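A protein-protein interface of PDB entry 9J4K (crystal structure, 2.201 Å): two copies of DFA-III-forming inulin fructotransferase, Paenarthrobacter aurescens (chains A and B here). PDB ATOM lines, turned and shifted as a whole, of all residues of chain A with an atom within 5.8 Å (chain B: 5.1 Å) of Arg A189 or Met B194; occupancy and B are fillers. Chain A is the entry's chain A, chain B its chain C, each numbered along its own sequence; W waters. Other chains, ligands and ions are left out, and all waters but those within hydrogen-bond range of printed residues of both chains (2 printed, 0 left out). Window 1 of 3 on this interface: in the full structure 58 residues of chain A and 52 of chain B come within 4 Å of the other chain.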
ATOM      1  N   ASP A 164      12.065  30.229 -15.878  1.00  0.00           N
ATOM      2  CA  ASP A 164      11.327  30.527 -14.627  1.00  0.00           C
ATOM      3  C   ASP A 164      11.661  29.442 -13.592  1.00  0.00           C
ATOM      4  O   ASP A 164      11.623  28.253 -13.941  1.00  0.00           O
ATOM      5  CB  ASP A 164       9.834  30.627 -14.931  1.00  0.00           C
ATOM      6  CG  ASP A 164       9.004  31.177 -13.790  1.00  0.00           C
ATOM      7  OD1 ASP A 164       9.532  32.033 -13.051  1.00  0.00           O
ATOM      8  OD2 ASP A 164       7.826  30.739 -13.658  1.00  0.00           O
ATOM      9  N   SER A 165      12.014  29.842 -12.370  1.00  0.00           N
ATOM     10  CA  SER A 165      12.100  28.945 -11.190  1.00  0.00           C
ATOM     11  C   SER A 165      13.162  27.861 -11.419  1.00  0.00           C
ATOM     12  O   SER A 165      12.954  26.712 -10.968  1.00  0.00           O
ATOM     13  CB  SER A 165      10.742  28.348 -10.876  1.00  0.00           C
ATOM     14  OG  SER A 165      10.639  28.030  -9.494  1.00  0.00           O
ATOM     15  N   ILE A 166      14.273  28.208 -12.072  1.00  0.00           N
ATOM     16  CA  ILE A 166      15.445  27.297 -12.162  1.00  0.00           C
ATOM     17  C   ILE A 166      16.157  27.318 -10.802  1.00  0.00           C
ATOM     18  O   ILE A 166      16.163  28.367 -10.137  1.00  0.00           O
ATOM     19  CB  ILE A 166      16.367  27.639 -13.347  1.00  0.00           C
ATOM     20  CG1 ILE A 166      15.696  27.293 -14.678  1.00  0.00           C
ATOM     21  CG2 ILE A 166      17.710  26.942 -13.205  1.00  0.00           C
ATOM     22  CD1 ILE A 166      16.595  27.419 -15.877  1.00  0.00           C
ATOM     23  N   HIS A 167      16.693  26.176 -10.385  1.00  0.00           N
ATOM     24  CA  HIS A 167      17.352  26.017  -9.068  1.00  0.00           C
ATOM     25  C   HIS A 167      18.706  25.338  -9.268  1.00  0.00           C
ATOM     26  O   HIS A 167      18.712  24.174  -9.725  1.00  0.00           O
ATOM     27  CB  HIS A 167      16.419  25.273  -8.113  1.00  0.00           C
ATOM     28  CG  HIS A 167      16.780  25.425  -6.674  1.00  0.00           C
ATOM     29  ND1 HIS A 167      16.236  24.617  -5.701  1.00  0.00           N
ATOM     30  CD2 HIS A 167      17.665  26.233  -6.047  1.00  0.00           C
ATOM     31  CE1 HIS A 167      16.735  24.944  -4.526  1.00  0.00           C
ATOM     32  NE2 HIS A 167      17.620  25.937  -4.712  1.00  0.00           N
ATOM     33  N   ILE A 168      19.786  26.072  -8.960  1.00  0.00           N
ATOM     34  CA  ILE A 168      21.204  25.617  -9.034  1.00  0.00           C
ATOM     35  C   ILE A 168      21.762  25.592  -7.607  1.00  0.00           C
ATOM     36  O   ILE A 168      21.985  26.667  -7.030  1.00  0.00           O
ATOM     37  CB  ILE A 168      22.053  26.536  -9.936  1.00  0.00           C
ATOM     38  CG1 ILE A 168      21.344  26.903 -11.243  1.00  0.00           C
ATOM     39  CG2 ILE A 168      23.419  25.909 -10.185  1.00  0.00           C
ATOM     40  CD1 ILE A 168      21.474  25.885 -12.335  1.00  0.00           C
ATOM     41  N   THR A 169      21.991  24.412  -7.048  1.00  0.00           N
ATOM     42  CA  THR A 169      22.391  24.296  -5.629  1.00  0.00           C
ATOM     43  C   THR A 169      23.361  23.130  -5.438  1.00  0.00           C
ATOM     44  O   THR A 169      23.242  22.137  -6.177  1.00  0.00           O
ATOM     45  CB  THR A 169      21.141  24.232  -4.747  1.00  0.00           C
ATOM     46  OG1 THR A 169      21.589  24.629  -3.458  1.00  0.00           O
ATOM     47  CG2 THR A 169      20.473  22.875  -4.723  1.00  0.00           C
ATOM     48  N   ALA A 187      12.889  34.392 -11.326  1.00  0.00           N
ATOM     49  CA  ALA A 187      12.695  33.587 -10.097  1.00  0.00           C
ATOM     50  C   ALA A 187      13.755  32.481 -10.059  1.00  0.00           C
ATOM     51  O   ALA A 187      13.415  31.347  -9.684  1.00  0.00           O
ATOM     52  CB  ALA A 187      11.293  33.026 -10.082  1.00  0.00           C
ATOM     53  N   LEU A 188      14.981  32.810 -10.485  1.00  0.00           N
ATOM     54  CA  LEU A 188      16.177  31.934 -10.437  1.00  0.00           C
ATOM     55  C   LEU A 188      16.760  31.991  -9.022  1.00  0.00           C
ATOM     56  O   LEU A 188      16.767  33.081  -8.417  1.00  0.00           O
ATOM     57  CB  LEU A 188      17.200  32.396 -11.484  1.00  0.00           C
ATOM     58  CG  LEU A 188      18.615  31.825 -11.355  1.00  0.00           C
ATOM     59  CD1 LEU A 188      18.674  30.377 -11.797  1.00  0.00           C
ATOM     60  CD2 LEU A 188      19.604  32.647 -12.158  1.00  0.00           C
ATOM     61  N   ARG A 189      17.222  30.845  -8.519  1.00  0.00           N
ATOM     62  CA  ARG A 189      17.986  30.733  -7.253  1.00  0.00           C
ATOM     63  C   ARG A 189      19.320  30.050  -7.564  1.00  0.00           C
ATOM     64  O   ARG A 189      19.312  28.877  -8.003  1.00  0.00           O
ATOM     65  CB  ARG A 189      17.188  29.962  -6.204  1.00  0.00           C
ATOM     66  CG  ARG A 189      16.075  30.763  -5.544  1.00  0.00           C
ATOM     67  CD  ARG A 189      15.162  29.842  -4.751  1.00  0.00           C
ATOM     68  NE  ARG A 189      14.419  28.908  -5.599  1.00  0.00           N
ATOM     69  CZ  ARG A 189      13.916  27.725  -5.216  1.00  0.00           C
ATOM     70  NH1 ARG A 189      14.103  27.259  -3.992  1.00  0.00           N
ATOM     71  NH2 ARG A 189      13.231  26.994  -6.072  1.00  0.00           N
ATOM     72  N   VAL A 190      20.412  30.799  -7.431  1.00  0.00           N
ATOM     73  CA  VAL A 190      21.804  30.265  -7.470  1.00  0.00           C
ATOM     74  C   VAL A 190      22.288  30.254  -6.015  1.00  0.00           C
ATOM     75  O   VAL A 190      22.682  31.320  -5.527  1.00  0.00           O
ATOM     76  CB  VAL A 190      22.707  31.104  -8.394  1.00  0.00           C
ATOM     77  CG1 VAL A 190      24.141  30.580  -8.416  1.00  0.00           C
ATOM     78  CG2 VAL A 190      22.154  31.168  -9.813  1.00  0.00           C
ATOM     79  N   HIS A 191      22.197  29.096  -5.352  1.00  0.00           N
ATOM     80  CA  HIS A 191      22.226  28.953  -3.872  1.00  0.00           C
ATOM     81  C   HIS A 191      23.205  27.852  -3.436  1.00  0.00           C
ATOM     82  O   HIS A 191      23.068  26.714  -3.914  1.00  0.00           O
ATOM     83  CB  HIS A 191      20.819  28.639  -3.349  1.00  0.00           C
ATOM     84  CG  HIS A 191      20.783  28.351  -1.890  1.00  0.00           C
ATOM     85  ND1 HIS A 191      20.904  29.349  -0.942  1.00  0.00           N
ATOM     86  CD2 HIS A 191      20.677  27.185  -1.222  1.00  0.00           C
ATOM     87  CE1 HIS A 191      20.858  28.801   0.255  1.00  0.00           C
ATOM     88  NE2 HIS A 191      20.740  27.478   0.105  1.00  0.00           N
ATOM     89  N   THR A 211      15.280  37.315  -8.732  1.00  0.00           N
ATOM     90  CA  THR A 211      16.351  36.295  -8.599  1.00  0.00           C
ATOM     91  C   THR A 211      17.036  36.419  -7.227  1.00  0.00           C
ATOM     92  O   THR A 211      17.088  37.537  -6.676  1.00  0.00           O
ATOM     93  CB  THR A 211      17.290  36.378  -9.806  1.00  0.00           C
ATOM     94  OG1 THR A 211      16.479  35.994 -10.918  1.00  0.00           O
ATOM     95  CG2 THR A 211      18.501  35.477  -9.689  1.00  0.00           C
ATOM     96  N   ILE A 212      17.506  35.291  -6.683  1.00  0.00           N
ATOM     97  CA  ILE A 212      18.369  35.247  -5.464  1.00  0.00           C
ATOM     98  C   ILE A 212      19.680  34.533  -5.802  1.00  0.00           C
ATOM     99  O   ILE A 212      19.648  33.421  -6.368  1.00  0.00           O
ATOM    100  CB  ILE A 212      17.675  34.581  -4.257  1.00  0.00           C
ATOM    101  CG1 ILE A 212      16.272  35.137  -4.011  1.00  0.00           C
ATOM    102  CG2 ILE A 212      18.549  34.711  -3.010  1.00  0.00           C
ATOM    103  CD1 ILE A 212      15.485  34.373  -2.959  1.00  0.00           C
ATOM    104  N   VAL A 213      20.798  35.173  -5.463  1.00  0.00           N
ATOM    105  CA  VAL A 213      22.147  34.547  -5.463  1.00  0.00           C
ATOM    106  C   VAL A 213      22.627  34.572  -4.008  1.00  0.00           C
ATOM    107  O   VAL A 213      22.936  35.668  -3.522  1.00  0.00           O
ATOM    108  CB  VAL A 213      23.120  35.272  -6.411  1.00  0.00           C
ATOM    109  CG1 VAL A 213      24.489  34.624  -6.379  1.00  0.00           C
ATOM    110  CG2 VAL A 213      22.590  35.340  -7.840  1.00  0.00           C
ATOM    111  N   HIS B  80      10.865  20.755  -7.339  1.00  0.00           N
ATOM    112  CA  HIS B  80       9.807  21.679  -6.859  1.00  0.00           C
ATOM    113  C   HIS B  80       8.757  21.933  -7.954  1.00  0.00           C
ATOM    114  O   HIS B  80       7.653  22.367  -7.599  1.00  0.00           O
ATOM    115  CB  HIS B  80      10.443  22.990  -6.382  1.00  0.00           C
ATOM    116  CG  HIS B  80      11.139  23.749  -7.457  1.00  0.00           C
ATOM    117  ND1 HIS B  80      12.279  23.275  -8.078  1.00  0.00           N
ATOM    118  CD2 HIS B  80      10.883  24.959  -7.998  1.00  0.00           C
ATOM    119  CE1 HIS B  80      12.683  24.157  -8.965  1.00  0.00           C
ATOM    120  NE2 HIS B  80      11.851  25.201  -8.927  1.00  0.00           N
ATOM    121  N   PHE B  82       7.800  24.107 -10.204  1.00  0.00           N
ATOM    122  CA  PHE B  82       6.964  25.330 -10.293  1.00  0.00           C
ATOM    123  C   PHE B  82       6.707  25.704 -11.764  1.00  0.00           C
ATOM    124  O   PHE B  82       7.640  25.663 -12.602  1.00  0.00           O
ATOM    125  CB  PHE B  82       7.565  26.507  -9.531  1.00  0.00           C
ATOM    126  CG  PHE B  82       6.649  27.704  -9.568  1.00  0.00           C
ATOM    127  CD1 PHE B  82       6.734  28.629 -10.598  1.00  0.00           C
ATOM    128  CD2 PHE B  82       5.647  27.856  -8.623  1.00  0.00           C
ATOM    129  CE1 PHE B  82       5.872  29.714 -10.647  1.00  0.00           C
ATOM    130  CE2 PHE B  82       4.782  28.934  -8.679  1.00  0.00           C
ATOM    131  CZ  PHE B  82       4.895  29.860  -9.691  1.00  0.00           C
ATOM    132  N   GLY B 170      13.384  23.401  -0.396  1.00  0.00           N
ATOM    133  CA  GLY B 170      13.380  22.999  -1.813  1.00  0.00           C
ATOM    134  C   GLY B 170      11.983  22.663  -2.315  1.00  0.00           C
ATOM    135  O   GLY B 170      11.886  21.956  -3.332  1.00  0.00           O
ATOM    136  N   MET B 171      10.937  23.150  -1.643  1.00  0.00           N
ATOM    137  CA  MET B 171       9.527  22.852  -2.007  1.00  0.00           C
ATOM    138  C   MET B 171       9.097  23.782  -3.157  1.00  0.00           C
ATOM    139  O   MET B 171       9.727  24.844  -3.352  1.00  0.00           O
ATOM    140  CB  MET B 171       8.575  23.039  -0.818  1.00  0.00           C
ATOM    141  CG  MET B 171       8.721  21.976   0.278  1.00  0.00           C
ATOM    142  SD  MET B 171       8.309  20.286  -0.254  1.00  0.00           S
ATOM    143  CE  MET B 171       6.568  20.448  -0.641  1.00  0.00           C
ATOM    144  N   GLY B 172       8.072  23.370  -3.902  1.00  0.00           N
ATOM    145  CA  GLY B 172       7.280  24.247  -4.782  1.00  0.00           C
ATOM    146  C   GLY B 172       5.837  24.225  -4.329  1.00  0.00           C
ATOM    147  O   GLY B 172       5.322  23.118  -4.103  1.00  0.00           O
ATOM    148  N   PHE B 173       5.233  25.394  -4.112  1.00  0.00           N
ATOM    149  CA  PHE B 173       3.784  25.546  -3.803  1.00  0.00           C
ATOM    150  C   PHE B 173       3.162  26.464  -4.849  1.00  0.00           C
ATOM    151  O   PHE B 173       3.692  27.575  -5.055  1.00  0.00           O
ATOM    152  CB  PHE B 173       3.542  26.160  -2.425  1.00  0.00           C
ATOM    153  CG  PHE B 173       4.123  25.413  -1.252  1.00  0.00           C
ATOM    154  CD1 PHE B 173       5.434  25.632  -0.851  1.00  0.00           C
ATOM    155  CD2 PHE B 173       3.343  24.532  -0.513  1.00  0.00           C
ATOM    156  CE1 PHE B 173       5.944  24.989   0.268  1.00  0.00           C
ATOM    157  CE2 PHE B 173       3.862  23.884   0.597  1.00  0.00           C
ATOM    158  CZ  PHE B 173       5.165  24.108   0.982  1.00  0.00           C
ATOM    159  N   ASP B 192      14.740  28.183   1.363  1.00  0.00           N
ATOM    160  CA  ASP B 192      15.007  27.922  -0.069  1.00  0.00           C
ATOM    161  C   ASP B 192      13.802  27.186  -0.670  1.00  0.00           C
ATOM    162  O   ASP B 192      13.986  26.099  -1.222  1.00  0.00           O
ATOM    163  CB  ASP B 192      16.322  27.151  -0.209  1.00  0.00           C
ATOM    164  CG  ASP B 192      16.829  27.089  -1.633  1.00  0.00           C
ATOM    165  OD1 ASP B 192      16.421  27.952  -2.435  1.00  0.00           O
ATOM    166  OD2 ASP B 192      17.585  26.160  -1.934  1.00  0.00           O
ATOM    167  N   ASN B 193      12.615  27.780  -0.563  1.00  0.00           N
ATOM    168  CA  ASN B 193      11.370  27.277  -1.198  1.00  0.00           C
ATOM    169  C   ASN B 193      10.884  28.280  -2.248  1.00  0.00           C
ATOM    170  O   ASN B 193      11.253  29.478  -2.178  1.00  0.00           O
ATOM    171  CB  ASN B 193      10.250  27.027  -0.183  1.00  0.00           C
ATOM    172  CG  ASN B 193      10.633  26.024   0.881  1.00  0.00           C
ATOM    173  OD1 ASN B 193      10.658  24.814   0.631  1.00  0.00           O
ATOM    174  ND2 ASN B 193      10.944  26.521   2.071  1.00  0.00           N
ATOM    175  N   MET B 194      10.087  27.774  -3.185  1.00  0.00           N
ATOM    176  CA  MET B 194       9.307  28.555  -4.175  1.00  0.00           C
ATOM    177  C   MET B 194       7.847  28.505  -3.721  1.00  0.00           C
ATOM    178  O   MET B 194       7.240  27.420  -3.805  1.00  0.00           O
ATOM    179  CB  MET B 194       9.444  27.943  -5.572  1.00  0.00           C
ATOM    180  CG  MET B 194       8.639  28.658  -6.645  1.00  0.00           C
ATOM    181  SD  MET B 194       9.519  30.089  -7.258  1.00  0.00           S
ATOM    182  CE  MET B 194       8.309  30.885  -8.315  1.00  0.00           C
ATOM    183  N   VAL B 195       7.328  29.606  -3.183  1.00  0.00           N
ATOM    184  CA  VAL B 195       5.933  29.682  -2.662  1.00  0.00           C
ATOM    185  C   VAL B 195       5.227  30.830  -3.383  1.00  0.00           C
ATOM    186  O   VAL B 195       5.263  31.956  -2.866  1.00  0.00           O
ATOM    187  CB  VAL B 195       5.912  29.851  -1.131  1.00  0.00           C
ATOM    188  CG1 VAL B 195       4.559  29.460  -0.557  1.00  0.00           C
ATOM    189  CG2 VAL B 195       7.024  29.052  -0.453  1.00  0.00           C
ATOM    190  N   ALA B 196       4.600  30.557  -4.532  1.00  0.00           N
ATOM    191  CA  ALA B 196       4.088  31.612  -5.433  1.00  0.00           C
ATOM    192  C   ALA B 196       2.730  31.245  -6.042  1.00  0.00           C
ATOM    193  O   ALA B 196       2.420  30.039  -6.193  1.00  0.00           O
ATOM    194  CB  ALA B 196       5.111  31.900  -6.497  1.00  0.00           C
ATOM    195  N   ASP B 215      15.860  32.639   2.287  1.00  0.00           N
ATOM    196  CA  ASP B 215      16.290  32.256   0.917  1.00  0.00           C
ATOM    197  C   ASP B 215      15.080  31.789   0.097  1.00  0.00           C
ATOM    198  O   ASP B 215      15.308  31.130  -0.928  1.00  0.00           O
ATOM    199  CB  ASP B 215      17.463  31.269   1.011  1.00  0.00           C
ATOM    200  CG  ASP B 215      18.685  31.901   1.677  1.00  0.00           C
ATOM    201  OD1 ASP B 215      18.900  33.119   1.481  1.00  0.00           O
ATOM    202  OD2 ASP B 215      19.409  31.193   2.407  1.00  0.00           O
ATOM    203  N   LEU B 217      11.624  32.460  -2.369  1.00  0.00           N
ATOM    204  CA  LEU B 217      10.843  33.253  -3.349  1.00  0.00           C
ATOM    205  C   LEU B 217       9.376  33.126  -2.953  1.00  0.00           C
ATOM    206  O   LEU B 217       8.891  31.984  -2.925  1.00  0.00           O
ATOM    207  CB  LEU B 217      11.068  32.679  -4.751  1.00  0.00           C
ATOM    208  CG  LEU B 217      12.460  32.896  -5.332  1.00  0.00           C
ATOM    209  CD1 LEU B 217      12.716  31.972  -6.511  1.00  0.00           C
ATOM    210  CD2 LEU B 217      12.636  34.341  -5.743  1.00  0.00           C
ATOM    211  N   PHE B 243       7.730  39.104  -3.721  1.00  0.00           N
ATOM    212  CA  PHE B 243       7.167  39.841  -4.883  1.00  0.00           C
ATOM    213  C   PHE B 243       5.643  39.816  -4.748  1.00  0.00           C
ATOM    214  O   PHE B 243       5.125  39.173  -3.833  1.00  0.00           O
ATOM    215  CB  PHE B 243       7.737  39.270  -6.189  1.00  0.00           C
ATOM    216  CG  PHE B 243       7.757  37.768  -6.271  1.00  0.00           C
ATOM    217  CD1 PHE B 243       6.612  37.061  -6.605  1.00  0.00           C
ATOM    218  CD2 PHE B 243       8.918  37.057  -6.005  1.00  0.00           C
ATOM    219  CE1 PHE B 243       6.623  35.678  -6.662  1.00  0.00           C
ATOM    220  CE2 PHE B 243       8.927  35.672  -6.070  1.00  0.00           C
ATOM    221  CZ  PHE B 243       7.780  34.987  -6.395  1.00  0.00           C
HETATM  222  O   HOH W   1      13.965  23.198  -5.764  1.00  0.00           O
HETATM  223  O   HOH W   2      12.376  24.966  -4.499  1.00  0.00           O
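Among the printed residues, merely in contact across the chains: Ala A187 with Leu B217 (3.3 Å), His A191 with Asp B192 (3.3 Å), Ser A165 with Phe B82 (3.4 Å), His A191 with Asp B215 (3.5 Å), Arg A189 with Leu B217 (3.6 Å), Arg A189 with His B80 (3.6 Å), Asp A164 with Phe B82 (3.7 Å), Arg A189 with Asn B193 (3.8 Å), Ile A212 with Asp B215 (3.8 Å), Arg A189 with Met B194 (3.9 Å), Ile A212 with Leu B217 (3.98 Å) and His A167 with His B80 (3.99 Å).
The backbone NH (N) of Phe B173 lies within hydrogen-bond range of the backbone carbonyl oxygen (O) of Met B194. N of Met B171 is in hydrogen-bond range of OD1 of Asn B193 (2.8 Å). O of Ile A168 is in hydrogen-bond range of N of His A191 (3.0 Å). The backbone carbonyl oxygen of Ala A187 lies close to the backbone NH of Ser A165 (3.4 Å). N of Val B195 sits at hydrogen-bond distance from O of Leu B217, 2.9 Å away. The backbone carbonyl oxygen of His A191 sits at hydrogen-bond distance from the side-chain hydroxyl of Thr A169, at 2.6 Å.
Water W1 lies within hydrogen-bond range of ND1 of His A167 (2.7 Å), ND1 of His B80 (2.9 Å) and O of Gly B170 (3.4 Å). Water W2 lies within hydrogen-bond range of NH2 of Arg A189, O of Met B171 and O of Gly B170.
Arg A189 touches just these residues of chain B: His B80 (3.6 Å), Asp B192 (2.9 Å), Asn B193 (3.8 Å), Met B194 (3.9 Å) and Leu B217 (3.6 Å). Of the printed residues of chain B, His A191 touches Asp B192 and Asp B215. Of the printed residues of chain A, His B80 touches Ser A165, His A167 and Arg A189. Printed residues of chain A within 4 Å of Phe B82: Asp A164 (3.7 Å) and Ser A165 (3.4 Å). Of the printed residues of chain A, Asp B215 touches His A191 and Ile A212. The nearest residue of chain B that does not touch Arg A189 is Asp B215 (4.04 Å). The nearest printed residue of chain B that does not touch Asp A164 is Met B194 (5.0 Å).
No position is printed for both chains. Of the 16 pairs that touch across the chains among the printed residues, none has its exchanged pair printed and touching as well.
Of the 14 printed residues of chain B, 7 touch a printed residue of chain A. Printed residues of chain B that touch a printed residue of chain A: His B80, Phe B82, Asp B192, Asn B193, Met B194, Asp B215 and Leu B217. Among the printed residues, 16 pairs touch across the chains.
The side-chain carboxylate of Asp B192 is in salt-bridge range of the guanidinium group of Arg A189. A ring nitrogen (NE2) of His B80 is in hydrogen-bond range of the backbone carbonyl oxygen (O) of Ser A165, at 2.8 Å. NE2 of His A167 lies within hydrogen-bond range of OD2 of Asp B192 (2.8 Å). The side-chain sulfur (SD) of Met B194 lies within hydrogen-bond range of the side-chain hydroxyl (OG) of Ser A165, at 3.2 Å.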
